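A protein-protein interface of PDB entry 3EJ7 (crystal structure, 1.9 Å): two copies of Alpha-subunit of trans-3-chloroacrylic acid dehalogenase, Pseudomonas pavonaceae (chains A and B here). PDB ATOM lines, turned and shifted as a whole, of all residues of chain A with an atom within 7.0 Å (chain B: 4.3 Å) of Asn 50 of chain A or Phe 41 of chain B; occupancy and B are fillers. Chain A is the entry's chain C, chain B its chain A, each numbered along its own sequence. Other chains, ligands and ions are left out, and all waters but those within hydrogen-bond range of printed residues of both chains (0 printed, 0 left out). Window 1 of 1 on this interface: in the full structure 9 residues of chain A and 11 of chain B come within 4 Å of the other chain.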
ATOM      1  N   TYR A  10       6.493  -4.014  -0.747  1.00  0.00           N
ATOM      2  CA  TYR A  10       5.273  -4.335   0.025  1.00  0.00           C
ATOM      3  C   TYR A  10       4.039  -4.059  -0.798  1.00  0.00           C
ATOM      4  O   TYR A  10       4.044  -3.191  -1.661  1.00  0.00           O
ATOM      5  CB  TYR A  10       5.139  -3.436   1.280  1.00  0.00           C
ATOM      6  CG  TYR A  10       5.928  -3.879   2.487  1.00  0.00           C
ATOM      7  CD1 TYR A  10       5.614  -5.062   3.170  1.00  0.00           C
ATOM      8  CD2 TYR A  10       6.971  -3.090   2.985  1.00  0.00           C
ATOM      9  CE1 TYR A  10       6.353  -5.465   4.305  1.00  0.00           C
ATOM     10  CE2 TYR A  10       7.706  -3.475   4.107  1.00  0.00           C
ATOM     11  CZ  TYR A  10       7.395  -4.658   4.760  1.00  0.00           C
ATOM     12  OH  TYR A  10       8.140  -5.035   5.864  1.00  0.00           O
ATOM     13  N   GLU A  45      10.130  -8.241   1.536  1.00  0.00           N
ATOM     14  CA  GLU A  45       9.401  -7.030   1.199  1.00  0.00           C
ATOM     15  C   GLU A  45      10.051  -5.804   1.841  1.00  0.00           C
ATOM     16  O   GLU A  45      10.580  -5.893   2.941  1.00  0.00           O
ATOM     17  CB  GLU A  45       7.968  -7.167   1.703  1.00  0.00           C
ATOM     18  CG  GLU A  45       7.168  -8.247   0.991  1.00  0.00           C
ATOM     19  CD  GLU A  45       5.796  -8.428   1.572  1.00  0.00           C
ATOM     20  OE1 GLU A  45       5.697  -9.096   2.626  1.00  0.00           O
ATOM     21  OE2 GLU A  45       4.816  -7.909   0.987  1.00  0.00           O
ATOM     22  N   GLY A  46       9.981  -4.660   1.167  1.00  0.00           N
ATOM     23  CA  GLY A  46      10.469  -3.396   1.743  1.00  0.00           C
ATOM     24  C   GLY A  46       9.596  -2.243   1.295  1.00  0.00           C
ATOM     25  O   GLY A  46       8.778  -2.396   0.385  1.00  0.00           O
ATOM     26  N   SER A  47       9.756  -1.088   1.922  1.00  0.00           N
ATOM     27  CA  SER A  47       9.046   0.094   1.487  1.00  0.00           C
ATOM     28  C   SER A  47       9.760   0.726   0.290  1.00  0.00           C
ATOM     29  O   SER A  47      10.915   0.400   0.002  1.00  0.00           O
ATOM     30  CB  SER A  47       8.855   1.093   2.647  1.00  0.00           C
ATOM     31  OG  SER A  47      10.085   1.659   3.056  1.00  0.00           O
ATOM     32  N   GLY A  48       9.057   1.627  -0.398  1.00  0.00           N
ATOM     33  CA  GLY A  48       9.550   2.238  -1.630  1.00  0.00           C
ATOM     34  C   GLY A  48      10.931   2.856  -1.539  1.00  0.00           C
ATOM     35  O   GLY A  48      11.753   2.675  -2.434  1.00  0.00           O
ATOM     36  N   ILE A  49      11.192   3.601  -0.466  1.00  0.00           N
ATOM     37  CA  ILE A  49      12.497   4.242  -0.301  1.00  0.00           C
ATOM     38  C   ILE A  49      13.648   3.194  -0.318  1.00  0.00           C
ATOM     39  O   ILE A  49      14.760   3.524  -0.696  1.00  0.00           O
ATOM     40  CB  ILE A  49      12.545   5.154   0.965  1.00  0.00           C
ATOM     41  CG1 ILE A  49      13.737   6.122   0.966  1.00  0.00           C
ATOM     42  CG2 ILE A  49      12.573   4.326   2.246  1.00  0.00           C
ATOM     43  CD1 ILE A  49      13.718   7.155  -0.085  1.00  0.00           C
ATOM     44  N   ASN A  50      13.358   1.942   0.045  1.00  0.00           N
ATOM     45  CA  ASN A  50      14.373   0.878   0.080  1.00  0.00           C
ATOM     46  C   ASN A  50      14.731   0.228  -1.264  1.00  0.00           C
ATOM     47  O   ASN A  50      15.531  -0.718  -1.297  1.00  0.00           O
ATOM     48  CB  ASN A  50      13.993  -0.191   1.090  1.00  0.00           C
ATOM     49  CG  ASN A  50      14.212   0.265   2.519  1.00  0.00           C
ATOM     50  OD1 ASN A  50      14.849   1.270   2.765  1.00  0.00           O
ATOM     51  ND2 ASN A  50      13.731  -0.517   3.474  1.00  0.00           N
ATOM     52  N   PHE A  51      14.103   0.695  -2.345  1.00  0.00           N
ATOM     53  CA  PHE A  51      14.353   0.150  -3.696  1.00  0.00           C
ATOM     54  C   PHE A  51      14.740   1.232  -4.674  1.00  0.00           C
ATOM     55  O   PHE A  51      14.162   2.322  -4.654  1.00  0.00           O
ATOM     56  CB  PHE A  51      13.094  -0.550  -4.235  1.00  0.00           C
ATOM     57  CG  PHE A  51      12.770  -1.804  -3.534  1.00  0.00           C
ATOM     58  CD1 PHE A  51      11.997  -1.797  -2.378  1.00  0.00           C
ATOM     59  CD2 PHE A  51      13.259  -3.017  -4.007  1.00  0.00           C
ATOM     60  CE1 PHE A  51      11.716  -2.979  -1.726  1.00  0.00           C
ATOM     61  CE2 PHE A  51      12.973  -4.190  -3.350  1.00  0.00           C
ATOM     62  CZ  PHE A  51      12.215  -4.174  -2.211  1.00  0.00           C
ATOM     63  N   VAL A  52      15.716   0.932  -5.528  1.00  0.00           N
ATOM     64  CA  VAL A  52      16.102   1.848  -6.587  1.00  0.00           C
ATOM     65  C   VAL A  52      16.060   1.038  -7.885  1.00  0.00           C
ATOM     66  O   VAL A  52      16.794   0.055  -8.034  1.00  0.00           O
ATOM     67  CB  VAL A  52      17.490   2.488  -6.343  1.00  0.00           C
ATOM     68  CG1 VAL A  52      17.856   3.423  -7.493  1.00  0.00           C
ATOM     69  CG2 VAL A  52      17.513   3.262  -5.043  1.00  0.00           C
ATOM     70  N   GLU A  53      15.149   1.426  -8.779  1.00  0.00           N
ATOM     71  CA  GLU A  53      14.864   0.698 -10.021  1.00  0.00           C
ATOM     72  C   GLU A  53      14.859   1.706 -11.150  1.00  0.00           C
ATOM     73  O   GLU A  53      14.182   2.738 -11.065  1.00  0.00           O
ATOM     74  CB  GLU A  53      13.496  -0.011  -9.967  1.00  0.00           C
ATOM     75  CG  GLU A  53      13.479  -1.401  -9.292  1.00  0.00           C
ATOM     76  CD  GLU A  53      12.070  -1.996  -9.159  1.00  0.00           C
ATOM     77  OE1 GLU A  53      11.078  -1.346  -9.588  1.00  0.00           O
ATOM     78  OE2 GLU A  53      11.952  -3.112  -8.617  1.00  0.00           O
ATOM     79  N   HIS A  57      14.386   5.862  -6.553  1.00  0.00           N
ATOM     80  CA  HIS A  57      13.719   5.253  -5.398  1.00  0.00           C
ATOM     81  C   HIS A  57      12.233   5.154  -5.711  1.00  0.00           C
ATOM     82  O   HIS A  57      11.680   6.032  -6.364  1.00  0.00           O
ATOM     83  CB  HIS A  57      13.927   6.094  -4.143  1.00  0.00           C
ATOM     84  CG  HIS A  57      15.345   6.155  -3.684  1.00  0.00           C
ATOM     85  ND1 HIS A  57      15.825   5.381  -2.650  1.00  0.00           N
ATOM     86  CD2 HIS A  57      16.388   6.905  -4.109  1.00  0.00           C
ATOM     87  CE1 HIS A  57      17.101   5.660  -2.452  1.00  0.00           C
ATOM     88  NE2 HIS A  57      17.468   6.573  -3.333  1.00  0.00           N
ATOM     89  N   LEU A  58      11.598   4.087  -5.253  1.00  0.00           N
ATOM     90  CA  LEU A  58      10.193   3.853  -5.554  1.00  0.00           C
ATOM     91  C   LEU A  58       9.320   4.680  -4.621  1.00  0.00           C
ATOM     92  O   LEU A  58       9.713   4.944  -3.482  1.00  0.00           O
ATOM     93  CB  LEU A  58       9.849   2.345  -5.409  1.00  0.00           C
ATOM     94  CG  LEU A  58      10.583   1.331  -6.315  1.00  0.00           C
ATOM     95  CD1 LEU A  58      10.040  -0.067  -6.155  1.00  0.00           C
ATOM     96  CD2 LEU A  58      10.559   1.735  -7.783  1.00  0.00           C
ATOM     97  N   ASP A  60       5.553   4.836  -2.504  1.00  0.00           N
ATOM     98  CA  ASP A  60       4.646   3.861  -1.903  1.00  0.00           C
ATOM     99  C   ASP A  60       3.216   4.132  -2.357  1.00  0.00           C
ATOM    100  O   ASP A  60       2.474   3.209  -2.693  1.00  0.00           O
ATOM    101  CB  ASP A  60       4.736   3.890  -0.374  1.00  0.00           C
ATOM    102  CG  ASP A  60       6.100   3.446   0.143  1.00  0.00           C
ATOM    103  OD1 ASP A  60       6.778   4.273   0.789  1.00  0.00           O
ATOM    104  OD2 ASP A  60       6.494   2.281  -0.100  1.00  0.00           O
ATOM    105  N   ILE B   4      22.760  -4.648  -6.506  1.00  0.00           N
ATOM    106  CA  ILE B   4      23.399  -4.320  -5.217  1.00  0.00           C
ATOM    107  C   ILE B   4      22.390  -4.449  -4.073  1.00  0.00           C
ATOM    108  O   ILE B   4      21.254  -4.003  -4.198  1.00  0.00           O
ATOM    109  CB  ILE B   4      23.935  -2.863  -5.244  1.00  0.00           C
ATOM    110  CG1 ILE B   4      24.593  -2.537  -6.587  1.00  0.00           C
ATOM    111  CG2 ILE B   4      24.866  -2.600  -4.049  1.00  0.00           C
ATOM    112  CD1 ILE B   4      24.832  -1.059  -6.832  1.00  0.00           C
ATOM    113  N   SER B   5      22.825  -5.032  -2.952  1.00  0.00           N
ATOM    114  CA  SER B   5      22.017  -5.088  -1.718  1.00  0.00           C
ATOM    115  C   SER B   5      22.822  -4.534  -0.544  1.00  0.00           C
ATOM    116  O   SER B   5      24.060  -4.665  -0.505  1.00  0.00           O
ATOM    117  CB  SER B   5      21.563  -6.521  -1.431  1.00  0.00           C
ATOM    118  OG  SER B   5      22.664  -7.373  -1.128  1.00  0.00           O
ATOM    119  N   CYS B   6      22.119  -3.922   0.404  1.00  0.00           N
ATOM    120  CA  CYS B   6      22.722  -3.478   1.629  1.00  0.00           C
ATOM    121  C   CYS B   6      21.833  -3.918   2.790  1.00  0.00           C
ATOM    122  O   CYS B   6      20.680  -3.477   2.903  1.00  0.00           O
ATOM    123  CB  CYS B   6      22.891  -1.959   1.602  1.00  0.00           C
ATOM    124  SG  CYS B   6      23.487  -1.230   3.199  1.00  0.00           S
ATOM    125  N   LYS B  17      19.432   7.488   2.936  1.00  0.00           N
ATOM    126  CA  LYS B  17      19.306   6.370   2.024  1.00  0.00           C
ATOM    127  C   LYS B  17      19.495   6.824   0.583  1.00  0.00           C
ATOM    128  O   LYS B  17      20.091   6.105  -0.235  1.00  0.00           O
ATOM    129  CB  LYS B  17      17.985   5.582   2.240  1.00  0.00           C
ATOM    130  CG  LYS B  17      17.853   4.937   3.638  1.00  0.00           C
ATOM    131  CD  LYS B  17      16.588   4.095   3.747  1.00  0.00           C
ATOM    132  CE  LYS B  17      16.449   3.462   5.102  1.00  0.00           C
ATOM    133  NZ  LYS B  17      15.083   2.845   5.230  1.00  0.00           N
ATOM    134  N   LEU B  20      23.209   7.328   0.078  1.00  0.00           N
ATOM    135  CA  LEU B  20      23.774   5.984  -0.059  1.00  0.00           C
ATOM    136  C   LEU B  20      23.625   5.427  -1.480  1.00  0.00           C
ATOM    137  O   LEU B  20      24.606   4.974  -2.101  1.00  0.00           O
ATOM    138  CB  LEU B  20      23.124   5.044   0.968  1.00  0.00           C
ATOM    139  CG  LEU B  20      23.632   3.611   0.936  1.00  0.00           C
ATOM    140  CD1 LEU B  20      25.138   3.604   1.274  1.00  0.00           C
ATOM    141  CD2 LEU B  20      22.818   2.667   1.844  1.00  0.00           C
ATOM    142  N   SER B  21      22.399   5.467  -1.995  1.00  0.00           N
ATOM    143  CA  SER B  21      22.119   5.006  -3.345  1.00  0.00           C
ATOM    144  C   SER B  21      22.800   5.844  -4.453  1.00  0.00           C
ATOM    145  O   SER B  21      23.276   5.288  -5.435  1.00  0.00           O
ATOM    146  CB  SER B  21      20.602   4.843  -3.553  1.00  0.00           C
ATOM    147  OG  SER B  21      19.973   6.048  -3.926  1.00  0.00           O
ATOM    148  N   LEU B  24      26.575   4.763  -4.274  1.00  0.00           N
ATOM    149  CA  LEU B  24      26.759   3.388  -4.748  1.00  0.00           C
ATOM    150  C   LEU B  24      26.467   3.278  -6.251  1.00  0.00           C
ATOM    151  O   LEU B  24      27.209   2.633  -6.967  1.00  0.00           O
ATOM    152  CB  LEU B  24      25.917   2.407  -3.931  1.00  0.00           C
ATOM    153  CG  LEU B  24      26.462   1.536  -2.789  1.00  0.00           C
ATOM    154  CD1 LEU B  24      27.897   1.819  -2.268  1.00  0.00           C
ATOM    155  CD2 LEU B  24      25.450   1.455  -1.645  1.00  0.00           C
ATOM    156  N   ILE B  39      21.485  -0.595 -12.830  1.00  0.00           N
ATOM    157  CA  ILE B  39      21.931  -1.039 -11.518  1.00  0.00           C
ATOM    158  C   ILE B  39      20.746  -1.056 -10.557  1.00  0.00           C
ATOM    159  O   ILE B  39      20.215   0.013 -10.233  1.00  0.00           O
ATOM    160  CB  ILE B  39      23.016  -0.074 -10.967  1.00  0.00           C
ATOM    161  CG1 ILE B  39      24.267  -0.077 -11.847  1.00  0.00           C
ATOM    162  CG2 ILE B  39      23.374  -0.435  -9.544  1.00  0.00           C
ATOM    163  CD1 ILE B  39      25.066   1.182 -11.727  1.00  0.00           C
ATOM    164  N   PHE B  40      20.306  -2.245 -10.141  1.00  0.00           N
ATOM    165  CA  PHE B  40      19.264  -2.403  -9.138  1.00  0.00           C
ATOM    166  C   PHE B  40      19.834  -2.295  -7.714  1.00  0.00           C
ATOM    167  O   PHE B  40      20.909  -2.830  -7.442  1.00  0.00           O
ATOM    168  CB  PHE B  40      18.556  -3.755  -9.312  1.00  0.00           C
ATOM    169  CG  PHE B  40      17.619  -4.104  -8.193  1.00  0.00           C
ATOM    170  CD1 PHE B  40      16.289  -3.672  -8.214  1.00  0.00           C
ATOM    171  CD2 PHE B  40      18.059  -4.859  -7.102  1.00  0.00           C
ATOM    172  CE1 PHE B  40      15.417  -4.004  -7.172  1.00  0.00           C
ATOM    173  CE2 PHE B  40      17.201  -5.183  -6.061  1.00  0.00           C
ATOM    174  CZ  PHE B  40      15.870  -4.750  -6.094  1.00  0.00           C
ATOM    175  N   PHE B  41      19.119  -1.621  -6.812  1.00  0.00           N
ATOM    176  CA  PHE B  41      19.577  -1.531  -5.422  1.00  0.00           C
ATOM    177  C   PHE B  41      18.397  -1.825  -4.461  1.00  0.00           C
ATOM    178  O   PHE B  41      17.289  -1.260  -4.627  1.00  0.00           O
ATOM    179  CB  PHE B  41      20.179  -0.138  -5.159  1.00  0.00           C
ATOM    180  CG  PHE B  41      20.758   0.054  -3.768  1.00  0.00           C
ATOM    181  CD1 PHE B  41      21.471  -0.968  -3.128  1.00  0.00           C
ATOM    182  CD2 PHE B  41      20.625   1.280  -3.116  1.00  0.00           C
ATOM    183  CE1 PHE B  41      22.019  -0.771  -1.841  1.00  0.00           C
ATOM    184  CE2 PHE B  41      21.176   1.499  -1.857  1.00  0.00           C
ATOM    185  CZ  PHE B  41      21.879   0.466  -1.212  1.00  0.00           C
ATOM    186  N   VAL B  42      18.644  -2.675  -3.465  1.00  0.00           N
ATOM    187  CA  VAL B  42      17.701  -2.922  -2.362  1.00  0.00           C
ATOM    188  C   VAL B  42      18.412  -2.731  -1.000  1.00  0.00           C
ATOM    189  O   VAL B  42      19.526  -3.233  -0.798  1.00  0.00           O
ATOM    190  CB  VAL B  42      16.992  -4.326  -2.431  1.00  0.00           C
ATOM    191  CG1 VAL B  42      17.986  -5.504  -2.300  1.00  0.00           C
ATOM    192  CG2 VAL B  42      15.924  -4.475  -1.342  1.00  0.00           C
ATOM    193  N   ILE B  43      17.759  -1.984  -0.105  1.00  0.00           N
ATOM    194  CA  ILE B  43      18.126  -1.887   1.314  1.00  0.00           C
ATOM    195  C   ILE B  43      17.245  -2.793   2.159  1.00  0.00           C
ATOM    196  O   ILE B  43      16.024  -2.727   2.077  1.00  0.00           O
ATOM    197  CB  ILE B  43      18.013  -0.422   1.828  1.00  0.00           C
ATOM    198  CG1 ILE B  43      18.993   0.479   1.047  1.00  0.00           C
ATOM    199  CG2 ILE B  43      18.251  -0.357   3.348  1.00  0.00           C
ATOM    200  CD1 ILE B  43      18.700   2.044   1.085  1.00  0.00           C
ATOM    201  N   GLU B  45      16.551  -3.718   6.148  1.00  0.00           N
ATOM    202  CA  GLU B  45      16.780  -3.229   7.508  1.00  0.00           C
ATOM    203  C   GLU B  45      16.196  -4.166   8.543  1.00  0.00           C
ATOM    204  O   GLU B  45      15.248  -4.937   8.274  1.00  0.00           O
ATOM    205  CB  GLU B  45      16.145  -1.847   7.719  1.00  0.00           C
ATOM    206  CG  GLU B  45      16.649  -0.757   6.832  1.00  0.00           C
ATOM    207  CD  GLU B  45      15.721   0.424   6.864  1.00  0.00           C
ATOM    208  OE1 GLU B  45      14.643   0.326   6.244  1.00  0.00           O
ATOM    209  OE2 GLU B  45      16.030   1.439   7.526  1.00  0.00           O
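OG of Ser 21 of chain B lies within hydrogen-bond range of NE2 of His 57 of chain A.
The side-chain amino group (NZ) of Lys 17 of chain B sits at hydrogen-bond distance from the side-chain amide oxygen (OD1) of Asn 50 of chain A (2.9 Å).
O of Asn 50 of chain A lies within hydrogen-bond range of N of Ile 43 of chain B (2.8 Å).
N of Val 52 of chain A is in hydrogen-bond range of O of Phe 41 of chain B (2.8 Å).
ND2 of Asn 50 of chain A sits at hydrogen-bond distance from OE1 of Glu 45 of chain B (3.0 Å).
ND1 of His 57 of chain A lies within hydrogen-bond range of O of Ile 49 of chain A, at 2.9 Å.
O of Phe 51 of chain A is in hydrogen-bond range of N of Leu 58 of chain A, at 3.2 Å.
N of Ile 4 of chain B lies within hydrogen-bond range of O of Phe 40 of chain B.
O of Ile 4 of chain B sits at hydrogen-bond distance from N of Val 42 of chain B, 3.0 Å away.
The side-chain amino group (NZ) of Lys 17 of chain B lies within salt-bridge range of the side-chain carboxylate (OE1) of Glu 45 of chain B (2.8 Å).
N of Cys 6 of chain B is in hydrogen-bond range of O of Val 42 of chain B.
Asn 50 of chain A touches Phe 41 of chain B.
CA of Val 42 of chain B touches O of Asn 50 of chain A (3.3 Å).
Phe 51 of chain A touches Phe 40 of chain B.
Phe 41 of chain B touches Phe 51 of chain A.
Val 42 of chain B touches Phe 51 of chain A (CG2 to CE2, 3.6 Å).
Val 52 of chain A touches Ser 21 of chain B (CG2 to CB, 3.8 Å).
CA of Phe 40 of chain B touches O of Val 52 of chain A, 3.7 Å away.
CG of Glu 53 of chain A touches CD1 of Phe 40 of chain B, 3.8 Å away.
His 57 of chain A touches Lys 17 of chain B.
Of chain B, only Lys 17, Phe 41, Val 42, Ile 43 and Glu 45 come within 4 Å of Asn 50 of chain A.
Of chain A, only Asn 50 (3.8 Å), Phe 51 (3.4 Å) and Val 52 (2.8 Å) come within 4 Å of Phe 41 of chain B.
Printed residues of chain A within 4 Å of Glu 45 of chain B: Asn 50 (3.0 Å).
Printed residues of chain A within 4 Å of Ile 43 of chain B: Asn 50.
Hydrophobic or aromatic side chains of chain B within 4 Å of the printed part of chain A: Phe 40, Phe 41, Val 42 and Ile 43.
Hydrophobic or aromatic side chains of chain A that line the printed part of chain B: Phe 51, Val 52 and His 57.
Among the printed residues, 14 pairs touch across the chains.
Among the printed residues, no Asp or Glu carboxylate lies within 4 Å of a Lys or Arg side-chain nitrogen of the other chain.
Position printed for both chains: 45.
Of the 14 pairs that touch across the chains among the printed residues, none has its exchanged pair printed and touching as well.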
